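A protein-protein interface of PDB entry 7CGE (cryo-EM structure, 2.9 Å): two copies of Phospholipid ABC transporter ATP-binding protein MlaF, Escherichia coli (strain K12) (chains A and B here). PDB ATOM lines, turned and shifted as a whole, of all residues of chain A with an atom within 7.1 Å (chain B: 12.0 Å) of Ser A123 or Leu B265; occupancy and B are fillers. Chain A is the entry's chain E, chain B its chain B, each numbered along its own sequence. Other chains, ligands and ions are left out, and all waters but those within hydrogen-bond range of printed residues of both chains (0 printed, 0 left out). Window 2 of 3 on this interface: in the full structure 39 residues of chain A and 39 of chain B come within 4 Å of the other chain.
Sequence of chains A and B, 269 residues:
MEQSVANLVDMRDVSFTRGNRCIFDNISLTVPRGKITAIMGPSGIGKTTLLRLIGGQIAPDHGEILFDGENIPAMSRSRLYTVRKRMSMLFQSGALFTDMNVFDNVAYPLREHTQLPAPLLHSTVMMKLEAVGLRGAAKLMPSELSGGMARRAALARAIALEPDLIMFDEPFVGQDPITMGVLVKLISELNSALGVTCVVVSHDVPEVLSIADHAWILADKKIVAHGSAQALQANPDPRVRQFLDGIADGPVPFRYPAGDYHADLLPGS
NH1 of Arg A135 is in hydrogen-bond range of O of Asp B260, at 3.3 Å. A ring nitrogen (ND1) of His A122 is in hydrogen-bond range of the backbone carbonyl oxygen (O) of Asp B264 (2.8 Å). OD2 of Asp B264 is in salt-bridge range of NH1 of Arg A135. The backbone carbonyl oxygen (O) of Leu B265 sits at hydrogen-bond distance from the side-chain hydroxyl (OG) of Ser A123 (2.6 Å).
Among the printed residues, merely in contact across the chains: Arg A135 with Ala B258 (3.6 Å), Met A127 with Leu B265 (3.8 Å), Arg A135 with Gly B259 (3.8 Å) and Met A126 with Asp B264 (3.9 Å).
Printed residues of chain B within 4 Å of Ser A123: Leu B265. Leu B265 touches just these residues of chain A: Ser A123 and Met A127. No residue of chain B comes within 4 Å of Pro A119. His A122 touches one residue of chain B. No residue of chain B comes within 4 Å of Thr A124. No residue of chain B comes within 4 Å of Val A125. Of chain B, only Asp B264 (3.9 Å) comes within 4 Å of Met A126. Met A127 touches one residue of chain B. Of the printed residues of chain B, Arg A135 touches Ala B258 (3.6 Å), Gly B259 (3.8 Å), Asp B260 (3.3 Å) and Asp B264 (2.7 Å). Of the printed residues of chain A, Asp B260 touches Arg A135. Of the printed residues of chain A, Asp B264 touches His A122, Met A126 and Arg A135. Of the printed residues of chain A, Ala B258 touches Arg A135 (3.6 Å). Of the printed residues of chain A, Gly B259 touches Arg A135.
Of the 11 printed residues of chain B, 5 touch a printed residue of chain A. Hydrophobic or aromatic side chains of chain B that line the printed part of chain A: Ala B258 and Leu B265. Hydrophobic or aromatic side chains of chain A within 4 Å of the printed part of chain B: His A122, Met A126 and Met A127. Among the printed residues, 8 pairs touch across the chains. Among the printed residues, Asp or Glu carboxylates within 4 Å of a Lys or Arg side-chain nitrogen of the other chain: Arg A135 with Asp B264.
No position is printed for both chains.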
ATOM      1  N   PHE A 103     -11.440  -7.677  -9.677  1.00  0.00           N
ATOM      2  CA  PHE A 103     -11.528  -8.881  -8.855  1.00  0.00           C
ATOM      3  C   PHE A 103     -10.226  -9.667  -8.877  1.00  0.00           C
ATOM      4  O   PHE A 103      -9.771 -10.150  -7.837  1.00  0.00           O
ATOM      5  CB  PHE A 103     -12.679  -9.761  -9.333  1.00  0.00           C
ATOM      6  CG  PHE A 103     -12.964 -10.938  -8.442  1.00  0.00           C
ATOM      7  CD1 PHE A 103     -13.818 -10.813  -7.371  1.00  0.00           C
ATOM      8  CD2 PHE A 103     -12.391 -12.175  -8.686  1.00  0.00           C
ATOM      9  CE1 PHE A 103     -14.086 -11.888  -6.555  1.00  0.00           C
ATOM     10  CE2 PHE A 103     -12.646 -13.244  -7.868  1.00  0.00           C
ATOM     11  CZ  PHE A 103     -13.497 -13.101  -6.805  1.00  0.00           C
ATOM     12  N   ALA A 118     -12.442 -22.337  -3.962  1.00  0.00           N
ATOM     13  CA  ALA A 118     -12.987 -21.299  -4.827  1.00  0.00           C
ATOM     14  C   ALA A 118     -14.162 -20.567  -4.171  1.00  0.00           C
ATOM     15  O   ALA A 118     -14.294 -19.359  -4.387  1.00  0.00           O
ATOM     16  CB  ALA A 118     -13.364 -21.873  -6.196  1.00  0.00           C
ATOM     17  N   PRO A 119     -15.031 -21.201  -3.379  1.00  0.00           N
ATOM     18  CA  PRO A 119     -15.733 -20.438  -2.348  1.00  0.00           C
ATOM     19  C   PRO A 119     -14.783 -20.179  -1.194  1.00  0.00           C
ATOM     20  O   PRO A 119     -13.778 -20.866  -1.044  1.00  0.00           O
ATOM     21  CB  PRO A 119     -16.883 -21.357  -1.929  1.00  0.00           C
ATOM     22  CG  PRO A 119     -17.051 -22.265  -3.048  1.00  0.00           C
ATOM     23  CD  PRO A 119     -15.677 -22.516  -3.542  1.00  0.00           C
ATOM     24  N   LEU A 120     -15.106 -19.137  -0.416  1.00  0.00           N
ATOM     25  CA  LEU A 120     -14.301 -18.474   0.621  1.00  0.00           C
ATOM     26  C   LEU A 120     -13.159 -17.655   0.034  1.00  0.00           C
ATOM     27  O   LEU A 120     -12.500 -16.914   0.761  1.00  0.00           O
ATOM     28  CB  LEU A 120     -13.719 -19.427   1.677  1.00  0.00           C
ATOM     29  CG  LEU A 120     -14.588 -20.464   2.363  1.00  0.00           C
ATOM     30  CD1 LEU A 120     -13.796 -21.109   3.466  1.00  0.00           C
ATOM     31  CD2 LEU A 120     -15.812 -19.807   2.917  1.00  0.00           C
ATOM     32  N   LEU A 121     -12.910 -17.770  -1.263  1.00  0.00           N
ATOM     33  CA  LEU A 121     -12.105 -16.797  -1.977  1.00  0.00           C
ATOM     34  C   LEU A 121     -12.970 -15.792  -2.697  1.00  0.00           C
ATOM     35  O   LEU A 121     -12.584 -14.633  -2.828  1.00  0.00           O
ATOM     36  CB  LEU A 121     -11.190 -17.490  -2.985  1.00  0.00           C
ATOM     37  CG  LEU A 121     -10.069 -16.644  -3.577  1.00  0.00           C
ATOM     38  CD1 LEU A 121      -9.286 -16.022  -2.468  1.00  0.00           C
ATOM     39  CD2 LEU A 121      -9.165 -17.483  -4.431  1.00  0.00           C
ATOM     40  N   HIS A 122     -14.142 -16.215  -3.149  1.00  0.00           N
ATOM     41  CA  HIS A 122     -15.108 -15.274  -3.687  1.00  0.00           C
ATOM     42  C   HIS A 122     -15.708 -14.418  -2.583  1.00  0.00           C
ATOM     43  O   HIS A 122     -15.975 -13.233  -2.788  1.00  0.00           O
ATOM     44  CB  HIS A 122     -16.190 -16.036  -4.436  1.00  0.00           C
ATOM     45  CG  HIS A 122     -16.987 -15.190  -5.369  1.00  0.00           C
ATOM     46  ND1 HIS A 122     -18.121 -14.516  -4.975  1.00  0.00           N
ATOM     47  CD2 HIS A 122     -16.821 -14.915  -6.681  1.00  0.00           C
ATOM     48  CE1 HIS A 122     -18.617 -13.858  -6.005  1.00  0.00           C
ATOM     49  NE2 HIS A 122     -17.846 -14.082  -7.051  1.00  0.00           N
ATOM     50  N   SER A 123     -15.909 -14.991  -1.402  1.00  0.00           N
ATOM     51  CA  SER A 123     -16.478 -14.226  -0.303  1.00  0.00           C
ATOM     52  C   SER A 123     -15.462 -13.301   0.340  1.00  0.00           C
ATOM     53  O   SER A 123     -15.836 -12.245   0.852  1.00  0.00           O
ATOM     54  CB  SER A 123     -17.047 -15.165   0.752  1.00  0.00           C
ATOM     55  OG  SER A 123     -18.092 -15.941   0.216  1.00  0.00           O
ATOM     56  N   THR A 124     -14.186 -13.678   0.336  1.00  0.00           N
ATOM     57  CA  THR A 124     -13.170 -12.848   0.969  1.00  0.00           C
ATOM     58  C   THR A 124     -12.870 -11.611   0.140  1.00  0.00           C
ATOM     59  O   THR A 124     -12.722 -10.517   0.688  1.00  0.00           O
ATOM     60  CB  THR A 124     -11.903 -13.663   1.193  1.00  0.00           C
ATOM     61  OG1 THR A 124     -12.241 -14.869   1.877  1.00  0.00           O
ATOM     62  CG2 THR A 124     -10.917 -12.907   2.035  1.00  0.00           C
ATOM     63  N   VAL A 125     -12.791 -11.757  -1.182  1.00  0.00           N
ATOM     64  CA  VAL A 125     -12.502 -10.619  -2.043  1.00  0.00           C
ATOM     65  C   VAL A 125     -13.687  -9.665  -2.094  1.00  0.00           C
ATOM     66  O   VAL A 125     -13.502  -8.445  -2.129  1.00  0.00           O
ATOM     67  CB  VAL A 125     -12.084 -11.126  -3.435  1.00  0.00           C
ATOM     68  CG1 VAL A 125     -11.857  -9.993  -4.397  1.00  0.00           C
ATOM     69  CG2 VAL A 125     -10.818 -11.912  -3.320  1.00  0.00           C
ATOM     70  N   MET A 126     -14.912 -10.184  -2.036  1.00  0.00           N
ATOM     71  CA  MET A 126     -16.081  -9.312  -2.028  1.00  0.00           C
ATOM     72  C   MET A 126     -16.216  -8.550  -0.721  1.00  0.00           C
ATOM     73  O   MET A 126     -16.780  -7.456  -0.704  1.00  0.00           O
ATOM     74  CB  MET A 126     -17.345 -10.117  -2.291  1.00  0.00           C
ATOM     75  CG  MET A 126     -17.537 -10.487  -3.733  1.00  0.00           C
ATOM     76  SD  MET A 126     -17.520  -9.068  -4.821  1.00  0.00           S
ATOM     77  CE  MET A 126     -17.202  -9.869  -6.377  1.00  0.00           C
ATOM     78  N   MET A 127     -15.707  -9.097   0.376  1.00  0.00           N
ATOM     79  CA  MET A 127     -15.696  -8.349   1.624  1.00  0.00           C
ATOM     80  C   MET A 127     -14.623  -7.274   1.614  1.00  0.00           C
ATOM     81  O   MET A 127     -14.839  -6.184   2.146  1.00  0.00           O
ATOM     82  CB  MET A 127     -15.492  -9.291   2.806  1.00  0.00           C
ATOM     83  CG  MET A 127     -16.748  -9.996   3.263  1.00  0.00           C
ATOM     84  SD  MET A 127     -16.437 -11.606   3.999  1.00  0.00           S
ATOM     85  CE  MET A 127     -16.059 -11.145   5.670  1.00  0.00           C
ATOM     86  N   LYS A 128     -13.465  -7.561   1.015  1.00  0.00           N
ATOM     87  CA  LYS A 128     -12.399  -6.568   0.928  1.00  0.00           C
ATOM     88  C   LYS A 128     -12.773  -5.434  -0.012  1.00  0.00           C
ATOM     89  O   LYS A 128     -12.437  -4.276   0.245  1.00  0.00           O
ATOM     90  CB  LYS A 128     -11.101  -7.215   0.456  1.00  0.00           C
ATOM     91  CG  LYS A 128     -10.506  -8.236   1.382  1.00  0.00           C
ATOM     92  CD  LYS A 128     -10.093  -7.623   2.676  1.00  0.00           C
ATOM     93  CE  LYS A 128      -9.550  -8.672   3.613  1.00  0.00           C
ATOM     94  NZ  LYS A 128      -8.743  -9.650   2.876  1.00  0.00           N
ATOM     95  N   ARG A 135     -17.388  -2.646  -4.616  1.00  0.00           N
ATOM     96  CA  ARG A 135     -17.918  -3.972  -4.907  1.00  0.00           C
ATOM     97  C   ARG A 135     -18.635  -4.009  -6.247  1.00  0.00           C
ATOM     98  O   ARG A 135     -18.656  -5.050  -6.909  1.00  0.00           O
ATOM     99  CB  ARG A 135     -18.855  -4.417  -3.793  1.00  0.00           C
ATOM    100  CG  ARG A 135     -19.139  -5.888  -3.809  1.00  0.00           C
ATOM    101  CD  ARG A 135     -19.963  -6.314  -2.623  1.00  0.00           C
ATOM    102  NE  ARG A 135     -21.124  -5.460  -2.422  1.00  0.00           N
ATOM    103  CZ  ARG A 135     -22.277  -5.613  -3.054  1.00  0.00           C
ATOM    104  NH1 ARG A 135     -22.429  -6.586  -3.938  1.00  0.00           N
ATOM    105  NH2 ARG A 135     -23.281  -4.793  -2.802  1.00  0.00           N
ATOM    106  N   ARG B 255     -20.158   4.880  -2.033  1.00  0.00           N
ATOM    107  CA  ARG B 255     -20.246   3.549  -2.606  1.00  0.00           C
ATOM    108  C   ARG B 255     -20.500   3.620  -4.101  1.00  0.00           C
ATOM    109  O   ARG B 255     -21.298   4.431  -4.572  1.00  0.00           O
ATOM    110  CB  ARG B 255     -21.369   2.766  -1.939  1.00  0.00           C
ATOM    111  CG  ARG B 255     -21.157   2.531  -0.473  1.00  0.00           C
ATOM    112  CD  ARG B 255     -20.205   1.394  -0.271  1.00  0.00           C
ATOM    113  NE  ARG B 255     -19.670   1.370   1.080  1.00  0.00           N
ATOM    114  CZ  ARG B 255     -20.220   0.706   2.079  1.00  0.00           C
ATOM    115  NH1 ARG B 255     -21.325   0.021   1.869  1.00  0.00           N
ATOM    116  NH2 ARG B 255     -19.669   0.733   3.282  1.00  0.00           N
ATOM    117  N   ALA B 258     -23.707  -0.742  -6.937  1.00  0.00           N
ATOM    118  CA  ALA B 258     -23.483  -2.173  -6.914  1.00  0.00           C
ATOM    119  C   ALA B 258     -24.808  -2.908  -7.020  1.00  0.00           C
ATOM    120  O   ALA B 258     -25.880  -2.308  -7.109  1.00  0.00           O
ATOM    121  CB  ALA B 258     -22.749  -2.575  -5.635  1.00  0.00           C
ATOM    122  N   GLY B 259     -24.725  -4.229  -6.985  1.00  0.00           N
ATOM    123  CA  GLY B 259     -25.918  -5.040  -6.910  1.00  0.00           C
ATOM    124  C   GLY B 259     -26.333  -5.180  -5.466  1.00  0.00           C
ATOM    125  O   GLY B 259     -26.520  -4.180  -4.769  1.00  0.00           O
ATOM    126  N   ASP B 260     -26.468  -6.409  -4.995  1.00  0.00           N
ATOM    127  CA  ASP B 260     -26.785  -6.656  -3.602  1.00  0.00           C
ATOM    128  C   ASP B 260     -25.842  -7.708  -3.049  1.00  0.00           C
ATOM    129  O   ASP B 260     -25.154  -8.409  -3.793  1.00  0.00           O
ATOM    130  CB  ASP B 260     -28.224  -7.126  -3.435  1.00  0.00           C
ATOM    131  CG  ASP B 260     -28.483  -8.423  -4.153  1.00  0.00           C
ATOM    132  OD1 ASP B 260     -27.906  -8.612  -5.244  1.00  0.00           O
ATOM    133  OD2 ASP B 260     -29.251  -9.255  -3.630  1.00  0.00           O
ATOM    134  N   TYR B 261     -25.849  -7.843  -1.729  1.00  0.00           N
ATOM    135  CA  TYR B 261     -25.208  -8.983  -1.110  1.00  0.00           C
ATOM    136  C   TYR B 261     -26.022 -10.252  -1.333  1.00  0.00           C
ATOM    137  O   TYR B 261     -27.018 -10.279  -2.061  1.00  0.00           O
ATOM    138  CB  TYR B 261     -25.092  -8.820   0.390  1.00  0.00           C
ATOM    139  CG  TYR B 261     -24.144  -7.806   0.927  1.00  0.00           C
ATOM    140  CD1 TYR B 261     -22.767  -7.979   0.842  1.00  0.00           C
ATOM    141  CD2 TYR B 261     -24.630  -6.728   1.632  1.00  0.00           C
ATOM    142  CE1 TYR B 261     -21.917  -7.071   1.400  1.00  0.00           C
ATOM    143  CE2 TYR B 261     -23.799  -5.826   2.185  1.00  0.00           C
ATOM    144  CZ  TYR B 261     -22.454  -5.998   2.070  1.00  0.00           C
ATOM    145  OH  TYR B 261     -21.681  -5.055   2.659  1.00  0.00           O
ATOM    146  N   HIS B 262     -25.568 -11.324  -0.685  1.00  0.00           N
ATOM    147  CA  HIS B 262     -26.183 -12.650  -0.673  1.00  0.00           C
ATOM    148  C   HIS B 262     -26.281 -13.274  -2.064  1.00  0.00           C
ATOM    149  O   HIS B 262     -26.984 -14.272  -2.244  1.00  0.00           O
ATOM    150  CB  HIS B 262     -27.565 -12.626   0.000  1.00  0.00           C
ATOM    151  CG  HIS B 262     -27.889 -13.875   0.754  1.00  0.00           C
ATOM    152  ND1 HIS B 262     -27.548 -14.054   2.076  1.00  0.00           N
ATOM    153  CD2 HIS B 262     -28.503 -15.017   0.365  1.00  0.00           C
ATOM    154  CE1 HIS B 262     -27.951 -15.247   2.474  1.00  0.00           C
ATOM    155  NE2 HIS B 262     -28.531 -15.853   1.454  1.00  0.00           N
ATOM    156  N   ALA B 263     -25.606 -12.708  -3.050  1.00  0.00           N
ATOM    157  CA  ALA B 263     -25.473 -13.272  -4.376  1.00  0.00           C
ATOM    158  C   ALA B 263     -24.028 -13.367  -4.808  1.00  0.00           C
ATOM    159  O   ALA B 263     -23.686 -14.253  -5.590  1.00  0.00           O
ATOM    160  CB  ALA B 263     -26.250 -12.434  -5.398  1.00  0.00           C
ATOM    161  N   ASP B 264     -23.178 -12.469  -4.317  1.00  0.00           N
ATOM    162  CA  ASP B 264     -21.734 -12.597  -4.414  1.00  0.00           C
ATOM    163  C   ASP B 264     -21.087 -12.954  -3.089  1.00  0.00           C
ATOM    164  O   ASP B 264     -20.027 -13.579  -3.082  1.00  0.00           O
ATOM    165  CB  ASP B 264     -21.123 -11.295  -4.935  1.00  0.00           C
ATOM    166  CG  ASP B 264     -21.740 -10.073  -4.304  1.00  0.00           C
ATOM    167  OD1 ASP B 264     -22.498 -10.226  -3.325  1.00  0.00           O
ATOM    168  OD2 ASP B 264     -21.474  -8.956  -4.791  1.00  0.00           O
ATOM    169  N   LEU B 265     -21.704 -12.569  -1.973  1.00  0.00           N
ATOM    170  CA  LEU B 265     -21.205 -12.988  -0.672  1.00  0.00           C
ATOM    171  C   LEU B 265     -21.445 -14.473  -0.448  1.00  0.00           C
ATOM    172  O   LEU B 265     -20.579 -15.174   0.083  1.00  0.00           O
ATOM    173  CB  LEU B 265     -21.875 -12.172   0.425  1.00  0.00           C
ATOM    174  CG  LEU B 265     -21.171 -12.117   1.770  1.00  0.00           C
ATOM    175  CD1 LEU B 265     -19.796 -11.543   1.582  1.00  0.00           C
ATOM    176  CD2 LEU B 265     -21.968 -11.266   2.724  1.00  0.00           C
ATOM    177  N   LEU B 266     -22.612 -14.969  -0.847  1.00  0.00           N
ATOM    178  CA  LEU B 266     -22.957 -16.387  -0.753  1.00  0.00           C
ATOM    179  C   LEU B 266     -23.527 -16.815  -2.096  1.00  0.00           C
ATOM    180  O   LEU B 266     -24.747 -16.939  -2.254  1.00  0.00           O
ATOM    181  CB  LEU B 266     -23.958 -16.642   0.372  1.00  0.00           C
ATOM    182  CG  LEU B 266     -23.430 -16.451   1.786  1.00  0.00           C
ATOM    183  CD1 LEU B 266     -24.565 -16.358   2.767  1.00  0.00           C
ATOM    184  CD2 LEU B 266     -22.537 -17.601   2.131  1.00  0.00           C
ATOM    185  N   PRO B 267     -22.668 -17.054  -3.094  1.00  0.00           N
ATOM    186  CA  PRO B 267     -23.154 -17.351  -4.441  1.00  0.00           C
ATOM    187  C   PRO B 267     -23.648 -18.780  -4.592  1.00  0.00           C
ATOM    188  O   PRO B 267     -24.257 -19.077  -5.616  1.00  0.00           O
ATOM    189  CB  PRO B 267     -21.923 -17.110  -5.307  1.00  0.00           C
ATOM    190  CG  PRO B 267     -20.793 -17.485  -4.426  1.00  0.00           C
ATOM    191  CD  PRO B 267     -21.199 -17.126  -3.018  1.00  0.00           C
